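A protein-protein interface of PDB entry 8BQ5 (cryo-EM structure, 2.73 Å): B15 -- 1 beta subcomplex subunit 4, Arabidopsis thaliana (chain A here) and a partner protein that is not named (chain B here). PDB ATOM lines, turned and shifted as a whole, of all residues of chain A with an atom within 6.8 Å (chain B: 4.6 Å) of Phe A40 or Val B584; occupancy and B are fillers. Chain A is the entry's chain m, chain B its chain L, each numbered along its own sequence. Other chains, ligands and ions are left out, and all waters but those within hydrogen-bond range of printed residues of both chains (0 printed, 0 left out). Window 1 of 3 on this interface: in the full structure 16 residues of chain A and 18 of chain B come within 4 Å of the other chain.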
ATOM      1  N   ARG A  32     -14.010  26.869  12.401  1.00  0.00           N
ATOM      2  CA  ARG A  32     -14.833  26.175  13.427  1.00  0.00           C
ATOM      3  C   ARG A  32     -14.382  26.632  14.812  1.00  0.00           C
ATOM      4  O   ARG A  32     -15.251  26.883  15.654  1.00  0.00           O
ATOM      5  CB  ARG A  32     -14.686  24.656  13.300  1.00  0.00           C
ATOM      6  CG  ARG A  32     -15.334  23.884  14.441  1.00  0.00           C
ATOM      7  CD  ARG A  32     -15.223  22.375  14.345  1.00  0.00           C
ATOM      8  NE  ARG A  32     -16.333  21.775  13.621  1.00  0.00           N
ATOM      9  CZ  ARG A  32     -17.469  21.372  14.181  1.00  0.00           C
ATOM     10  NH1 ARG A  32     -17.651  21.496  15.485  1.00  0.00           N
ATOM     11  NH2 ARG A  32     -18.422  20.840  13.434  1.00  0.00           N
ATOM     12  N   ALA A  35     -15.411  30.211  15.621  1.00  0.00           N
ATOM     13  CA  ALA A  35     -16.818  30.305  15.988  1.00  0.00           C
ATOM     14  C   ALA A  35     -17.070  29.736  17.379  1.00  0.00           C
ATOM     15  O   ALA A  35     -17.778  30.346  18.186  1.00  0.00           O
ATOM     16  CB  ALA A  35     -17.678  29.587  14.948  1.00  0.00           C
ATOM     17  N   LEU A  36     -16.494  28.567  17.677  1.00  0.00           N
ATOM     18  CA  LEU A  36     -16.717  27.942  18.977  1.00  0.00           C
ATOM     19  C   LEU A  36     -16.177  28.806  20.108  1.00  0.00           C
ATOM     20  O   LEU A  36     -16.851  29.002  21.125  1.00  0.00           O
ATOM     21  CB  LEU A  36     -16.068  26.561  19.015  1.00  0.00           C
ATOM     22  CG  LEU A  36     -16.696  25.459  18.160  1.00  0.00           C
ATOM     23  CD1 LEU A  36     -15.942  24.152  18.350  1.00  0.00           C
ATOM     24  CD2 LEU A  36     -18.165  25.291  18.492  1.00  0.00           C
ATOM     25  N   ILE A  37     -14.958  29.324  19.952  1.00  0.00           N
ATOM     26  CA  ILE A  37     -14.381  30.188  20.975  1.00  0.00           C
ATOM     27  C   ILE A  37     -15.143  31.505  21.051  1.00  0.00           C
ATOM     28  O   ILE A  37     -15.318  32.075  22.134  1.00  0.00           O
ATOM     29  CB  ILE A  37     -12.881  30.399  20.705  1.00  0.00           C
ATOM     30  CG1 ILE A  37     -12.155  29.054  20.761  1.00  0.00           C
ATOM     31  CG2 ILE A  37     -12.282  31.368  21.709  1.00  0.00           C
ATOM     32  CD1 ILE A  37     -10.730  29.104  20.290  1.00  0.00           C
ATOM     33  N   GLY A  38     -15.608  32.008  19.909  1.00  0.00           N
ATOM     34  CA  GLY A  38     -16.420  33.212  19.928  1.00  0.00           C
ATOM     35  C   GLY A  38     -17.758  33.008  20.614  1.00  0.00           C
ATOM     36  O   GLY A  38     -18.178  33.829  21.431  1.00  0.00           O
ATOM     37  N   ILE A  39     -18.441  31.908  20.299  1.00  0.00           N
ATOM     38  CA  ILE A  39     -19.775  31.680  20.847  1.00  0.00           C
ATOM     39  C   ILE A  39     -19.702  31.255  22.307  1.00  0.00           C
ATOM     40  O   ILE A  39     -20.429  31.776  23.159  1.00  0.00           O
ATOM     41  CB  ILE A  39     -20.534  30.640  20.002  1.00  0.00           C
ATOM     42  CG1 ILE A  39     -20.898  31.221  18.637  1.00  0.00           C
ATOM     43  CG2 ILE A  39     -21.790  30.182  20.727  1.00  0.00           C
ATOM     44  CD1 ILE A  39     -21.008  30.184  17.545  1.00  0.00           C
ATOM     45  N   PHE A  40     -18.819  30.308  22.620  1.00  0.00           N
ATOM     46  CA  PHE A  40     -18.836  29.651  23.917  1.00  0.00           C
ATOM     47  C   PHE A  40     -17.730  30.110  24.854  1.00  0.00           C
ATOM     48  O   PHE A  40     -17.727  29.709  26.022  1.00  0.00           O
ATOM     49  CB  PHE A  40     -18.749  28.135  23.723  1.00  0.00           C
ATOM     50  CG  PHE A  40     -20.008  27.535  23.176  1.00  0.00           C
ATOM     51  CD1 PHE A  40     -21.197  27.645  23.872  1.00  0.00           C
ATOM     52  CD2 PHE A  40     -20.011  26.895  21.949  1.00  0.00           C
ATOM     53  CE1 PHE A  40     -22.360  27.105  23.370  1.00  0.00           C
ATOM     54  CE2 PHE A  40     -21.174  26.355  21.439  1.00  0.00           C
ATOM     55  CZ  PHE A  40     -22.350  26.460  22.152  1.00  0.00           C
ATOM     56  N   GLY A  41     -16.803  30.935  24.385  1.00  0.00           N
ATOM     57  CA  GLY A  41     -15.757  31.429  25.254  1.00  0.00           C
ATOM     58  C   GLY A  41     -15.952  32.881  25.625  1.00  0.00           C
ATOM     59  O   GLY A  41     -15.429  33.348  26.642  1.00  0.00           O
ATOM     60  N   ILE A  42     -16.713  33.608  24.809  1.00  0.00           N
ATOM     61  CA  ILE A  42     -16.909  35.036  25.015  1.00  0.00           C
ATOM     62  C   ILE A  42     -18.397  35.352  25.111  1.00  0.00           C
ATOM     63  O   ILE A  42     -18.851  35.938  26.099  1.00  0.00           O
ATOM     64  CB  ILE A  42     -16.246  35.854  23.889  1.00  0.00           C
ATOM     65  CG1 ILE A  42     -14.884  35.256  23.520  1.00  0.00           C
ATOM     66  CG2 ILE A  42     -16.095  37.304  24.310  1.00  0.00           C
ATOM     67  CD1 ILE A  42     -14.017  36.162  22.677  1.00  0.00           C
ATOM     68  N   ALA A  43     -19.162  34.969  24.086  1.00  0.00           N
ATOM     69  CA  ALA A  43     -20.556  35.394  23.994  1.00  0.00           C
ATOM     70  C   ALA A  43     -21.401  34.817  25.125  1.00  0.00           C
ATOM     71  O   ALA A  43     -22.089  35.555  25.838  1.00  0.00           O
ATOM     72  CB  ALA A  43     -21.135  34.996  22.636  1.00  0.00           C
ATOM     73  N   LEU A  44     -21.363  33.495  25.305  1.00  0.00           N
ATOM     74  CA  LEU A  44     -22.181  32.868  26.342  1.00  0.00           C
ATOM     75  C   LEU A  44     -21.829  33.344  27.746  1.00  0.00           C
ATOM     76  O   LEU A  44     -22.757  33.625  28.524  1.00  0.00           O
ATOM     77  CB  LEU A  44     -22.096  31.342  26.227  1.00  0.00           C
ATOM     78  CG  LEU A  44     -23.081  30.568  27.109  1.00  0.00           C
ATOM     79  CD1 LEU A  44     -24.458  31.225  27.107  1.00  0.00           C
ATOM     80  CD2 LEU A  44     -23.180  29.112  26.681  1.00  0.00           C
ATOM     81  N   PRO A  45     -20.555  33.446  28.148  1.00  0.00           N
ATOM     82  CA  PRO A  45     -20.274  34.054  29.460  1.00  0.00           C
ATOM     83  C   PRO A  45     -20.837  35.457  29.610  1.00  0.00           C
ATOM     84  O   PRO A  45     -21.328  35.807  30.689  1.00  0.00           O
ATOM     85  CB  PRO A  45     -18.739  34.043  29.526  1.00  0.00           C
ATOM     86  CG  PRO A  45     -18.344  32.910  28.668  1.00  0.00           C
ATOM     87  CD  PRO A  45     -19.330  32.894  27.537  1.00  0.00           C
ATOM     88  N   ARG B 579     -21.441  15.922  22.653  1.00  0.00           N
ATOM     89  CA  ARG B 579     -20.494  16.508  21.709  1.00  0.00           C
ATOM     90  C   ARG B 579     -19.900  17.803  22.243  1.00  0.00           C
ATOM     91  O   ARG B 579     -18.744  18.127  21.949  1.00  0.00           O
ATOM     92  CB  ARG B 579     -21.169  16.753  20.363  1.00  0.00           C
ATOM     93  CG  ARG B 579     -21.323  15.520  19.502  1.00  0.00           C
ATOM     94  CD  ARG B 579     -21.856  15.906  18.138  1.00  0.00           C
ATOM     95  NE  ARG B 579     -20.981  16.870  17.483  1.00  0.00           N
ATOM     96  CZ  ARG B 579     -21.343  17.648  16.474  1.00  0.00           C
ATOM     97  NH1 ARG B 579     -22.567  17.607  15.973  1.00  0.00           N
ATOM     98  NH2 ARG B 579     -20.456  18.491  15.954  1.00  0.00           N
ATOM     99  N   PHE B 580     -20.678  18.567  23.011  1.00  0.00           N
ATOM    100  CA  PHE B 580     -20.155  19.795  23.599  1.00  0.00           C
ATOM    101  C   PHE B 580     -18.986  19.499  24.529  1.00  0.00           C
ATOM    102  O   PHE B 580     -17.971  20.205  24.514  1.00  0.00           O
ATOM    103  CB  PHE B 580     -21.268  20.534  24.348  1.00  0.00           C
ATOM    104  CG  PHE B 580     -20.836  21.847  24.948  1.00  0.00           C
ATOM    105  CD1 PHE B 580     -20.236  21.894  26.197  1.00  0.00           C
ATOM    106  CD2 PHE B 580     -21.036  23.033  24.267  1.00  0.00           C
ATOM    107  CE1 PHE B 580     -19.842  23.096  26.751  1.00  0.00           C
ATOM    108  CE2 PHE B 580     -20.642  24.240  24.817  1.00  0.00           C
ATOM    109  CZ  PHE B 580     -20.044  24.270  26.061  1.00  0.00           C
ATOM    110  N   TYR B 582     -16.648  17.322  24.624  1.00  0.00           N
ATOM    111  CA  TYR B 582     -15.354  17.018  24.027  1.00  0.00           C
ATOM    112  C   TYR B 582     -14.902  18.121  23.074  1.00  0.00           C
ATOM    113  O   TYR B 582     -13.790  18.639  23.200  1.00  0.00           O
ATOM    114  CB  TYR B 582     -15.417  15.666  23.307  1.00  0.00           C
ATOM    115  CG  TYR B 582     -14.118  15.264  22.652  1.00  0.00           C
ATOM    116  CD1 TYR B 582     -13.110  14.657  23.390  1.00  0.00           C
ATOM    117  CD2 TYR B 582     -13.896  15.485  21.300  1.00  0.00           C
ATOM    118  CE1 TYR B 582     -11.921  14.289  22.805  1.00  0.00           C
ATOM    119  CE2 TYR B 582     -12.706  15.118  20.704  1.00  0.00           C
ATOM    120  CZ  TYR B 582     -11.722  14.519  21.462  1.00  0.00           C
ATOM    121  OH  TYR B 582     -10.532  14.147  20.883  1.00  0.00           O
ATOM    122  N   GLU B 583     -15.765  18.506  22.131  1.00  0.00           N
ATOM    123  CA  GLU B 583     -15.339  19.379  21.043  1.00  0.00           C
ATOM    124  C   GLU B 583     -15.252  20.847  21.439  1.00  0.00           C
ATOM    125  O   GLU B 583     -14.599  21.620  20.732  1.00  0.00           O
ATOM    126  CB  GLU B 583     -16.282  19.241  19.850  1.00  0.00           C
ATOM    127  CG  GLU B 583     -16.238  17.887  19.180  1.00  0.00           C
ATOM    128  CD  GLU B 583     -17.459  17.635  18.330  1.00  0.00           C
ATOM    129  OE1 GLU B 583     -17.659  18.385  17.352  1.00  0.00           O
ATOM    130  OE2 GLU B 583     -18.219  16.695  18.638  1.00  0.00           O
ATOM    131  N   VAL B 584     -15.891  21.261  22.529  1.00  0.00           N
ATOM    132  CA  VAL B 584     -15.913  22.683  22.849  1.00  0.00           C
ATOM    133  C   VAL B 584     -15.243  22.950  24.189  1.00  0.00           C
ATOM    134  O   VAL B 584     -14.216  23.634  24.253  1.00  0.00           O
ATOM    135  CB  VAL B 584     -17.351  23.230  22.846  1.00  0.00           C
ATOM    136  CG1 VAL B 584     -17.336  24.720  23.117  1.00  0.00           C
ATOM    137  CG2 VAL B 584     -18.031  22.932  21.522  1.00  0.00           C
ATOM    138  N   SER B 585     -15.814  22.414  25.267  1.00  0.00           N
ATOM    139  CA  SER B 585     -15.303  22.739  26.595  1.00  0.00           C
ATOM    140  C   SER B 585     -13.913  22.155  26.809  1.00  0.00           C
ATOM    141  O   SER B 585     -13.097  22.725  27.541  1.00  0.00           O
ATOM    142  CB  SER B 585     -16.276  22.251  27.669  1.00  0.00           C
ATOM    143  OG  SER B 585     -16.378  20.839  27.672  1.00  0.00           O
ATOM    144  N   PHE B 586     -13.616  21.029  26.161  1.00  0.00           N
ATOM    145  CA  PHE B 586     -12.319  20.378  26.299  1.00  0.00           C
ATOM    146  C   PHE B 586     -11.367  20.727  25.158  1.00  0.00           C
ATOM    147  O   PHE B 586     -10.261  21.220  25.397  1.00  0.00           O
ATOM    148  CB  PHE B 586     -12.504  18.859  26.388  1.00  0.00           C
ATOM    149  CG  PHE B 586     -11.224  18.109  26.595  1.00  0.00           C
ATOM    150  CD1 PHE B 586     -10.431  18.357  27.703  1.00  0.00           C
ATOM    151  CD2 PHE B 586     -10.809  17.158  25.680  1.00  0.00           C
ATOM    152  CE1 PHE B 586      -9.251  17.669  27.893  1.00  0.00           C
ATOM    153  CE2 PHE B 586      -9.630  16.469  25.866  1.00  0.00           C
ATOM    154  CZ  PHE B 586      -8.851  16.722  26.974  1.00  0.00           C
ATOM    155  N   GLU B 587     -11.781  20.479  23.915  1.00  0.00           N
ATOM    156  CA  GLU B 587     -10.868  20.602  22.784  1.00  0.00           C
ATOM    157  C   GLU B 587     -10.718  22.051  22.331  1.00  0.00           C
ATOM    158  O   GLU B 587      -9.601  22.514  22.078  1.00  0.00           O
ATOM    159  CB  GLU B 587     -11.351  19.720  21.631  1.00  0.00           C
ATOM    160  CG  GLU B 587     -10.435  19.696  20.424  1.00  0.00           C
ATOM    161  CD  GLU B 587     -10.814  18.616  19.428  1.00  0.00           C
ATOM    162  OE1 GLU B 587     -12.005  18.526  19.063  1.00  0.00           O
ATOM    163  OE2 GLU B 587      -9.918  17.851  19.013  1.00  0.00           O
ATOM    164  N   ALA B 588     -11.829  22.780  22.213  1.00  0.00           N
ATOM    165  CA  ALA B 588     -11.744  24.163  21.757  1.00  0.00           C
ATOM    166  C   ALA B 588     -11.208  25.081  22.849  1.00  0.00           C
ATOM    167  O   ALA B 588     -10.409  25.982  22.569  1.00  0.00           O
ATOM    168  CB  ALA B 588     -13.109  24.647  21.269  1.00  0.00           C
ATOM    169  N   LEU B 589     -11.635  24.877  24.093  1.00  0.00           N
ATOM    170  CA  LEU B 589     -11.246  25.797  25.154  1.00  0.00           C
ATOM    171  C   LEU B 589     -10.102  25.267  26.009  1.00  0.00           C
ATOM    172  O   LEU B 589      -9.024  25.864  26.034  1.00  0.00           O
ATOM    173  CB  LEU B 589     -12.451  26.120  26.038  1.00  0.00           C
ATOM    174  CG  LEU B 589     -13.602  26.821  25.321  1.00  0.00           C
ATOM    175  CD1 LEU B 589     -14.869  26.793  26.160  1.00  0.00           C
ATOM    176  CD2 LEU B 589     -13.206  28.248  24.989  1.00  0.00           C
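NE of Arg B579 lies within salt-bridge range of OE2 of Glu B583, at 3.0 Å.
N of Ser B585 sits at hydrogen-bond distance from O of Phe B580, 3.2 Å away.
The backbone NH (N) of Ala B588 sits at hydrogen-bond distance from the backbone carbonyl oxygen (O) of Glu B583.
The backbone NH of Leu B589 lies within hydrogen-bond range of the backbone carbonyl oxygen of Val B584 (2.9 Å).
The backbone carbonyl oxygen of Ile A37 sits at hydrogen-bond distance from the backbone NH of Ile A42, at 3.4 Å.
Among the printed residues, merely in contact across the chains: Phe A40 with Phe B580 (3.6 Å), Phe A40 with Val B584 (3.6 Å), Leu A36 with Glu B583 (3.7 Å), Leu A36 with Val B584 (3.8 Å) and Ile A37 with Ala B588 (3.9 Å).
Of the 10 printed residues of chain B, 4 touch a printed residue of chain A.
Among the printed residues, 6 pairs touch across the chains.
Among the printed residues, Asp or Glu carboxylates within 4 Å of a Lys or Arg side-chain nitrogen of the other chain: Arg A32 with Glu B583.
The side-chain carboxylate (OE1) of Glu B583 lies within salt-bridge range of the guanidinium group (NH1) of Arg A32 (3.6 Å).
Of the printed residues of chain B, Arg A32 touches Glu B583.
Printed residues of chain B within 4 Å of Leu A36: Glu B583 and Val B584.
Ile A39 touches none of the printed residues of chain B.
Of chain B, only Phe B580 (3.6 Å) and Val B584 (3.6 Å) come within 4 Å of Phe A40.
Printed residues of chain A within 4 Å of Phe B580: Phe A40.
Leu B589 touches none of the printed residues of chain A.
The nearest residue of chain B that does not touch Phe A40 is Leu B589 (4.1 Å).
The nearest residue of chain A that does not touch Val B584 is Ile A37 (6.1 Å).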
